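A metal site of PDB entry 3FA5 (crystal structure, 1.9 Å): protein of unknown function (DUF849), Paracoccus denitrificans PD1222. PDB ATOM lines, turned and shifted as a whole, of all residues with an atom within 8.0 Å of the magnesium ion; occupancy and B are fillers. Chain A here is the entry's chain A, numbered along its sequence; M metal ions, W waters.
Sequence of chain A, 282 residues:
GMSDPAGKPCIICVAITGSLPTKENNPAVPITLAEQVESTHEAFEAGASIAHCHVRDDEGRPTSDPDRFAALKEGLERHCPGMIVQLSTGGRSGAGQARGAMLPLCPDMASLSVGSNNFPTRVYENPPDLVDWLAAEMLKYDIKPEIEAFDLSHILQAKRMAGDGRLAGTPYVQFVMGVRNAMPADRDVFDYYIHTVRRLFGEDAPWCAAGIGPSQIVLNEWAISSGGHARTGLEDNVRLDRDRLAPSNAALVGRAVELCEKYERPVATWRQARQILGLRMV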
ATOM      1  N   ALA A  15       2.577   7.600  10.842  1.00  0.00           N
ATOM      2  CA  ALA A  15       2.897   8.750   9.967  1.00  0.00           C
ATOM      3  C   ALA A  15       1.971   8.655   8.735  1.00  0.00           C
ATOM      4  O   ALA A  15       2.143   7.828   7.871  1.00  0.00           O
ATOM      5  CB  ALA A  15       4.395   8.695   9.559  1.00  0.00           C
ATOM      6  N   ILE A  16       0.952   9.498   8.687  1.00  0.00           N
ATOM      7  CA  ILE A  16      -0.244   9.215   7.905  1.00  0.00           C
ATOM      8  C   ILE A  16      -0.145   9.530   6.378  1.00  0.00           C
ATOM      9  O   ILE A  16      -0.766   8.846   5.578  1.00  0.00           O
ATOM     10  CB  ILE A  16      -1.479   9.947   8.511  1.00  0.00           C
ATOM     11  CG1 ILE A  16      -1.309  11.458   8.446  1.00  0.00           C
ATOM     12  CG2 ILE A  16      -1.775   9.435   9.930  1.00  0.00           C
ATOM     13  CD1 ILE A  16      -2.571  12.204   8.861  1.00  0.00           C
ATOM     14  N   THR A  17       0.669  10.511   6.001  1.00  0.00           N
ATOM     15  CA  THR A  17       0.602  11.144   4.683  1.00  0.00           C
ATOM     16  C   THR A  17       1.994  11.435   4.081  1.00  0.00           C
ATOM     17  O   THR A  17       2.274  11.081   2.922  1.00  0.00           O
ATOM     18  CB  THR A  17      -0.196  12.473   4.765  1.00  0.00           C
ATOM     19  OG1 THR A  17      -1.552  12.203   5.164  1.00  0.00           O
ATOM     20  CG2 THR A  17      -0.241  13.160   3.371  1.00  0.00           C
ATOM     21  N   GLY A  18       2.873  12.035   4.870  1.00  0.00           N
ATOM     22  CA  GLY A  18       4.141  12.430   4.354  1.00  0.00           C
ATOM     23  C   GLY A  18       4.071  13.446   3.223  1.00  0.00           C
ATOM     24  O   GLY A  18       3.055  14.095   3.011  1.00  0.00           O
ATOM     25  N   SER A  19       5.181  13.579   2.516  1.00  0.00           N
ATOM     26  CA  SER A  19       5.356  14.629   1.515  1.00  0.00           C
ATOM     27  C   SER A  19       5.254  14.113   0.102  1.00  0.00           C
ATOM     28  O   SER A  19       4.778  14.839  -0.777  1.00  0.00           O
ATOM     29  CB  SER A  19       6.716  15.304   1.706  1.00  0.00           C
ATOM     30  OG  SER A  19       6.641  16.261   2.739  1.00  0.00           O
ATOM     31  N   HIS A  52       1.823  11.485  13.309  1.00  0.00           N
ATOM     32  CA  HIS A  52       2.863  12.333  12.727  1.00  0.00           C
ATOM     33  C   HIS A  52       2.271  12.882  11.457  1.00  0.00           C
ATOM     34  O   HIS A  52       2.005  12.126  10.532  1.00  0.00           O
ATOM     35  CB  HIS A  52       4.131  11.554  12.441  1.00  0.00           C
ATOM     36  CG  HIS A  52       5.120  12.302  11.629  1.00  0.00           C
ATOM     37  ND1 HIS A  52       6.105  13.087  12.184  1.00  0.00           N
ATOM     38  CD2 HIS A  52       5.301  12.379  10.283  1.00  0.00           C
ATOM     39  CE1 HIS A  52       6.842  13.612  11.226  1.00  0.00           C
ATOM     40  NE2 HIS A  52       6.390  13.186  10.063  1.00  0.00           N
ATOM     41  N   CYS A  53       2.017  14.195  11.476  1.00  0.00           N
ATOM     42  CA  CYS A  53       1.294  14.884  10.425  1.00  0.00           C
ATOM     43  C   CYS A  53       2.056  15.758   9.433  1.00  0.00           C
ATOM     44  O   CYS A  53       2.746  16.713   9.855  1.00  0.00           O
ATOM     45  CB  CYS A  53       0.367  15.873  11.085  1.00  0.00           C
ATOM     46  SG  CYS A  53      -0.791  15.016  12.144  1.00  0.00           S
ATOM     47  N   HIS A  54       1.874  15.486   8.143  1.00  0.00           N
ATOM     48  CA  HIS A  54       2.140  16.486   7.091  1.00  0.00           C
ATOM     49  C   HIS A  54       0.798  17.004   6.518  1.00  0.00           C
ATOM     50  O   HIS A  54      -0.265  16.379   6.703  1.00  0.00           O
ATOM     51  CB  HIS A  54       2.956  15.919   5.918  1.00  0.00           C
ATOM     52  CG  HIS A  54       4.343  15.434   6.258  1.00  0.00           C
ATOM     53  ND1 HIS A  54       5.440  15.725   5.476  1.00  0.00           N
ATOM     54  CD2 HIS A  54       4.790  14.599   7.223  1.00  0.00           C
ATOM     55  CE1 HIS A  54       6.510  15.127   5.965  1.00  0.00           C
ATOM     56  NE2 HIS A  54       6.147  14.433   7.046  1.00  0.00           N
ATOM     57  N   GLN A  86       1.651  15.333  16.515  1.00  0.00           N
ATOM     58  CA  GLN A  86       3.033  15.654  16.160  1.00  0.00           C
ATOM     59  C   GLN A  86       3.139  16.280  14.774  1.00  0.00           C
ATOM     60  O   GLN A  86       2.849  15.638  13.772  1.00  0.00           O
ATOM     61  CB  GLN A  86       3.906  14.384  16.204  1.00  0.00           C
ATOM     62  CG  GLN A  86       5.370  14.700  15.915  1.00  0.00           C
ATOM     63  CD  GLN A  86       6.178  13.493  15.916  1.00  0.00           C
ATOM     64  OE1 GLN A  86       6.625  13.046  14.866  1.00  0.00           O
ATOM     65  NE2 GLN A  86       6.365  12.919  17.108  1.00  0.00           N
ATOM     66  N   LEU A  87       3.536  17.554  14.696  1.00  0.00           N
ATOM     67  CA  LEU A  87       3.563  18.225  13.412  1.00  0.00           C
ATOM     68  C   LEU A  87       4.989  18.150  12.783  1.00  0.00           C
ATOM     69  O   LEU A  87       5.992  18.281  13.482  1.00  0.00           O
ATOM     70  CB  LEU A  87       3.072  19.684  13.535  1.00  0.00           C
ATOM     71  CG  LEU A  87       1.715  19.916  14.184  1.00  0.00           C
ATOM     72  CD1 LEU A  87       1.370  21.364  14.086  1.00  0.00           C
ATOM     73  CD2 LEU A  87       0.604  19.061  13.564  1.00  0.00           C
ATOM     74  N   SER A  88       5.039  17.962  11.464  1.00  0.00           N
ATOM     75  CA  SER A  88       6.296  17.874  10.706  1.00  0.00           C
ATOM     76  C   SER A  88       6.933  19.250  10.491  1.00  0.00           C
ATOM     77  O   SER A  88       6.234  20.188  10.110  1.00  0.00           O
ATOM     78  CB  SER A  88       6.044  17.224   9.339  1.00  0.00           C
ATOM     79  OG  SER A  88       7.226  17.175   8.540  1.00  0.00           O
ATOM     80  N   THR A  89       8.237  19.363  10.780  1.00  0.00           N
ATOM     81  CA  THR A  89       9.069  20.503  10.356  1.00  0.00           C
ATOM     82  C   THR A  89       9.951  20.089   9.161  1.00  0.00           C
ATOM     83  O   THR A  89      11.033  20.633   8.938  1.00  0.00           O
ATOM     84  CB  THR A  89       9.960  20.990  11.513  1.00  0.00           C
ATOM     85  OG1 THR A  89      10.859  19.922  11.918  1.00  0.00           O
ATOM     86  CG2 THR A  89       9.064  21.471  12.683  1.00  0.00           C
ATOM     87  N   GLY A  90       9.469  19.123   8.386  1.00  0.00           N
ATOM     88  CA  GLY A  90      10.239  18.537   7.288  1.00  0.00           C
ATOM     89  C   GLY A  90      10.595  19.507   6.175  1.00  0.00           C
ATOM     90  O   GLY A  90       9.864  20.463   5.902  1.00  0.00           O
ATOM     91  N   GLY A  91      11.756  19.254   5.569  1.00  0.00           N
ATOM     92  CA  GLY A  91      12.372  20.147   4.565  1.00  0.00           C
ATOM     93  C   GLY A  91      11.945  19.892   3.126  1.00  0.00           C
ATOM     94  O   GLY A  91      12.337  20.645   2.239  1.00  0.00           O
ATOM     95  N   ARG A  92      11.143  18.843   2.910  1.00  0.00           N
ATOM     96  CA  ARG A  92      10.485  18.592   1.621  1.00  0.00           C
ATOM     97  C   ARG A  92       9.242  19.467   1.395  1.00  0.00           C
ATOM     98  O   ARG A  92       8.901  19.761   0.260  1.00  0.00           O
ATOM     99  CB  ARG A  92      10.077  17.127   1.472  1.00  0.00           C
ATOM    100  CG  ARG A  92      11.233  16.190   1.169  1.00  0.00           C
ATOM    101  CD  ARG A  92      10.771  14.931   0.448  1.00  0.00           C
ATOM    102  NE  ARG A  92      10.888  13.692   1.222  1.00  0.00           N
ATOM    103  CZ  ARG A  92      11.697  12.658   0.941  1.00  0.00           C
ATOM    104  NH1 ARG A  92      12.498  12.686  -0.108  1.00  0.00           N
ATOM    105  NH2 ARG A  92      11.702  11.586   1.732  1.00  0.00           N
ATOM    106  N   SER A  93       8.597  19.891   2.473  1.00  0.00           N
ATOM    107  CA  SER A  93       7.377  20.727   2.376  1.00  0.00           C
ATOM    108  C   SER A  93       7.609  22.227   2.570  1.00  0.00           C
ATOM    109  O   SER A  93       6.661  22.998   2.529  1.00  0.00           O
ATOM    110  CB  SER A  93       6.355  20.240   3.407  1.00  0.00           C
ATOM    111  OG  SER A  93       6.180  18.833   3.317  1.00  0.00           O
ATOM    112  N   SER A 111       8.363  16.897  14.841  1.00  0.00           N
ATOM    113  CA  SER A 111       9.585  16.231  14.380  1.00  0.00           C
ATOM    114  C   SER A 111      10.732  17.257  14.248  1.00  0.00           C
ATOM    115  O   SER A 111      10.487  18.454  13.990  1.00  0.00           O
ATOM    116  CB  SER A 111       9.310  15.566  13.045  1.00  0.00           C
ATOM    117  OG  SER A 111       9.011  16.557  12.073  1.00  0.00           O
ATOM    118  N   TYR A 124      19.656  16.203   2.047  1.00  0.00           N
ATOM    119  CA  TYR A 124      18.558  16.582   2.939  1.00  0.00           C
ATOM    120  C   TYR A 124      19.119  17.657   3.787  1.00  0.00           C
ATOM    121  O   TYR A 124      19.816  17.390   4.697  1.00  0.00           O
ATOM    122  CB  TYR A 124      18.040  15.396   3.786  1.00  0.00           C
ATOM    123  CG  TYR A 124      16.836  15.735   4.674  1.00  0.00           C
ATOM    124  CD1 TYR A 124      15.805  16.511   4.184  1.00  0.00           C
ATOM    125  CD2 TYR A 124      16.727  15.292   6.011  1.00  0.00           C
ATOM    126  CE1 TYR A 124      14.707  16.853   4.950  1.00  0.00           C
ATOM    127  CE2 TYR A 124      15.589  15.624   6.795  1.00  0.00           C
ATOM    128  CZ  TYR A 124      14.609  16.432   6.236  1.00  0.00           C
ATOM    129  OH  TYR A 124      13.467  16.818   6.881  1.00  0.00           O
ATOM    130  N   GLU A 148      14.541  13.019  14.502  1.00  0.00           N
ATOM    131  CA  GLU A 148      14.549  12.052  13.424  1.00  0.00           C
ATOM    132  C   GLU A 148      16.019  11.886  13.026  1.00  0.00           C
ATOM    133  O   GLU A 148      16.585  12.708  12.321  1.00  0.00           O
ATOM    134  CB  GLU A 148      13.697  12.533  12.254  1.00  0.00           C
ATOM    135  CG  GLU A 148      12.269  12.783  12.651  1.00  0.00           C
ATOM    136  CD  GLU A 148      11.337  12.991  11.469  1.00  0.00           C
ATOM    137  OE1 GLU A 148      11.715  13.727  10.527  1.00  0.00           O
ATOM    138  OE2 GLU A 148      10.202  12.422  11.498  1.00  0.00           O
ATOM    139  N   PHE A 150      18.836  10.280  11.182  1.00  0.00           N
ATOM    140  CA  PHE A 150      19.229   9.601   9.939  1.00  0.00           C
ATOM    141  C   PHE A 150      20.661   9.059   9.938  1.00  0.00           C
ATOM    142  O   PHE A 150      21.045   8.339   8.982  1.00  0.00           O
ATOM    143  CB  PHE A 150      19.093  10.531   8.712  1.00  0.00           C
ATOM    144  CG  PHE A 150      17.681  10.843   8.371  1.00  0.00           C
ATOM    145  CD1 PHE A 150      16.951  10.012   7.546  1.00  0.00           C
ATOM    146  CD2 PHE A 150      17.055  11.963   8.925  1.00  0.00           C
ATOM    147  CE1 PHE A 150      15.636  10.281   7.252  1.00  0.00           C
ATOM    148  CE2 PHE A 150      15.736  12.252   8.644  1.00  0.00           C
ATOM    149  CZ  PHE A 150      15.017  11.403   7.798  1.00  0.00           C
ATOM    150  N   GLN A 174      14.306   9.051  17.184  1.00  0.00           N
ATOM    151  CA  GLN A 174      13.805   8.050  16.242  1.00  0.00           C
ATOM    152  C   GLN A 174      14.957   7.590  15.303  1.00  0.00           C
ATOM    153  O   GLN A 174      15.524   8.381  14.593  1.00  0.00           O
ATOM    154  CB  GLN A 174      12.665   8.665  15.423  1.00  0.00           C
ATOM    155  CG  GLN A 174      11.957   7.740  14.454  1.00  0.00           C
ATOM    156  CD  GLN A 174      11.296   8.463  13.304  1.00  0.00           C
ATOM    157  OE1 GLN A 174      11.556   8.156  12.150  1.00  0.00           O
ATOM    158  NE2 GLN A 174      10.425   9.387  13.617  1.00  0.00           N
ATOM    159  N   ARG A 231       7.185   3.231  14.937  1.00  0.00           N
ATOM    160  CA  ARG A 231       6.571   4.132  13.964  1.00  0.00           C
ATOM    161  C   ARG A 231       6.170   3.323  12.746  1.00  0.00           C
ATOM    162  O   ARG A 231       6.867   2.366  12.361  1.00  0.00           O
ATOM    163  CB  ARG A 231       7.525   5.266  13.560  1.00  0.00           C
ATOM    164  CG  ARG A 231       7.025   6.084  12.364  1.00  0.00           C
ATOM    165  CD  ARG A 231       7.644   7.482  12.270  1.00  0.00           C
ATOM    166  NE  ARG A 231       7.696   7.926  10.872  1.00  0.00           N
ATOM    167  CZ  ARG A 231       7.731   9.184  10.463  1.00  0.00           C
ATOM    168  NH1 ARG A 231       7.731  10.185  11.318  1.00  0.00           N
ATOM    169  NH2 ARG A 231       7.774   9.454   9.171  1.00  0.00           N
ATOM    170  N   GLU A 235       3.236   7.187   5.116  1.00  0.00           N
ATOM    171  CA  GLU A 235       4.331   8.118   4.844  1.00  0.00           C
ATOM    172  C   GLU A 235       5.595   7.354   4.480  1.00  0.00           C
ATOM    173  O   GLU A 235       6.340   7.803   3.632  1.00  0.00           O
ATOM    174  CB  GLU A 235       4.576   9.007   6.053  1.00  0.00           C
ATOM    175  CG  GLU A 235       5.837   9.881   5.987  1.00  0.00           C
ATOM    176  CD  GLU A 235       5.739  11.044   6.908  1.00  0.00           C
ATOM    177  OE1 GLU A 235       4.623  11.394   7.320  1.00  0.00           O
ATOM    178  OE2 GLU A 235       6.778  11.646   7.239  1.00  0.00           O
ATOM    179  N   ASP A 236       5.836   6.205   5.111  1.00  0.00           N
ATOM    180  CA  ASP A 236       7.123   5.532   4.966  1.00  0.00           C
ATOM    181  C   ASP A 236       7.098   4.334   4.041  1.00  0.00           C
ATOM    182  O   ASP A 236       8.170   3.886   3.575  1.00  0.00           O
ATOM    183  CB  ASP A 236       7.654   5.075   6.333  1.00  0.00           C
ATOM    184  CG  ASP A 236       7.876   6.216   7.306  1.00  0.00           C
ATOM    185  OD1 ASP A 236       8.119   7.368   6.919  1.00  0.00           O
ATOM    186  OD2 ASP A 236       7.810   5.945   8.501  1.00  0.00           O
HETATM  187 MG    MG M   1       7.557  13.066   8.148  1.00  0.00          MG
HETATM  188  O   HOH W   1       9.031  12.236   8.995  1.00  0.00           O
HETATM  189  O   HOH W   2       9.003  13.367   6.398  1.00  0.00           O
HETATM  190  O   HOH W   3       8.395  14.758   8.736  1.00  0.00           O
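The side-chain carboxylate of Glu 148 lies within salt-bridge range of the guanidinium group of Arg 231.
N of Gly 18 sits at hydrogen-bond distance from OE1 of Glu 235, at 3.1 Å.
The guanidinium group of Arg 231 is in salt-bridge range of the side-chain carboxylate of Asp 236 (3.1 Å).
The side-chain carboxylate (OE2) of Glu 235 sits close to the guanidinium group (NH2) of Arg 231 (3.1 Å).
O of His 52 sits at hydrogen-bond distance from N of Ile 16, 3.4 Å away.
ND1 of His 54 is in hydrogen-bond range of OG of Ser 19.
The side-chain amide oxygen (OE1) of Gln 86 is in hydrogen-bond range of a ring nitrogen (ND1) of His 52 (2.7 Å).
N of Glu 235 is in hydrogen-bond range of O of Ala 15 (3.0 Å).
Residues that only touch the magnesium ion: Arg 231.
The nearest printed residue that does not touch the magnesium ion is Ser 88 (4.1 Å).
The magnesium ion is bound by the side-chain carboxylate (OE2) of Glu 235 (1.9 Å).
Water W1 binds the magnesium ion (1.9 Å).
Water W3 is bound to the magnesium ion, 2.0 Å away.
NE2 of His 52 binds the magnesium ion (2.2 Å).
The magnesium ion is bound by NE2 of His 54 (2.3 Å).
The magnesium ion is bound by water W2, 2.3 Å away.
The magnesium ion has six donor atoms within binding distance.
Water W1 lies within hydrogen-bond range of the side-chain carboxylate of Glu 148 (2.8 Å) and the guanidinium group of Arg 231 (3.1 Å).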
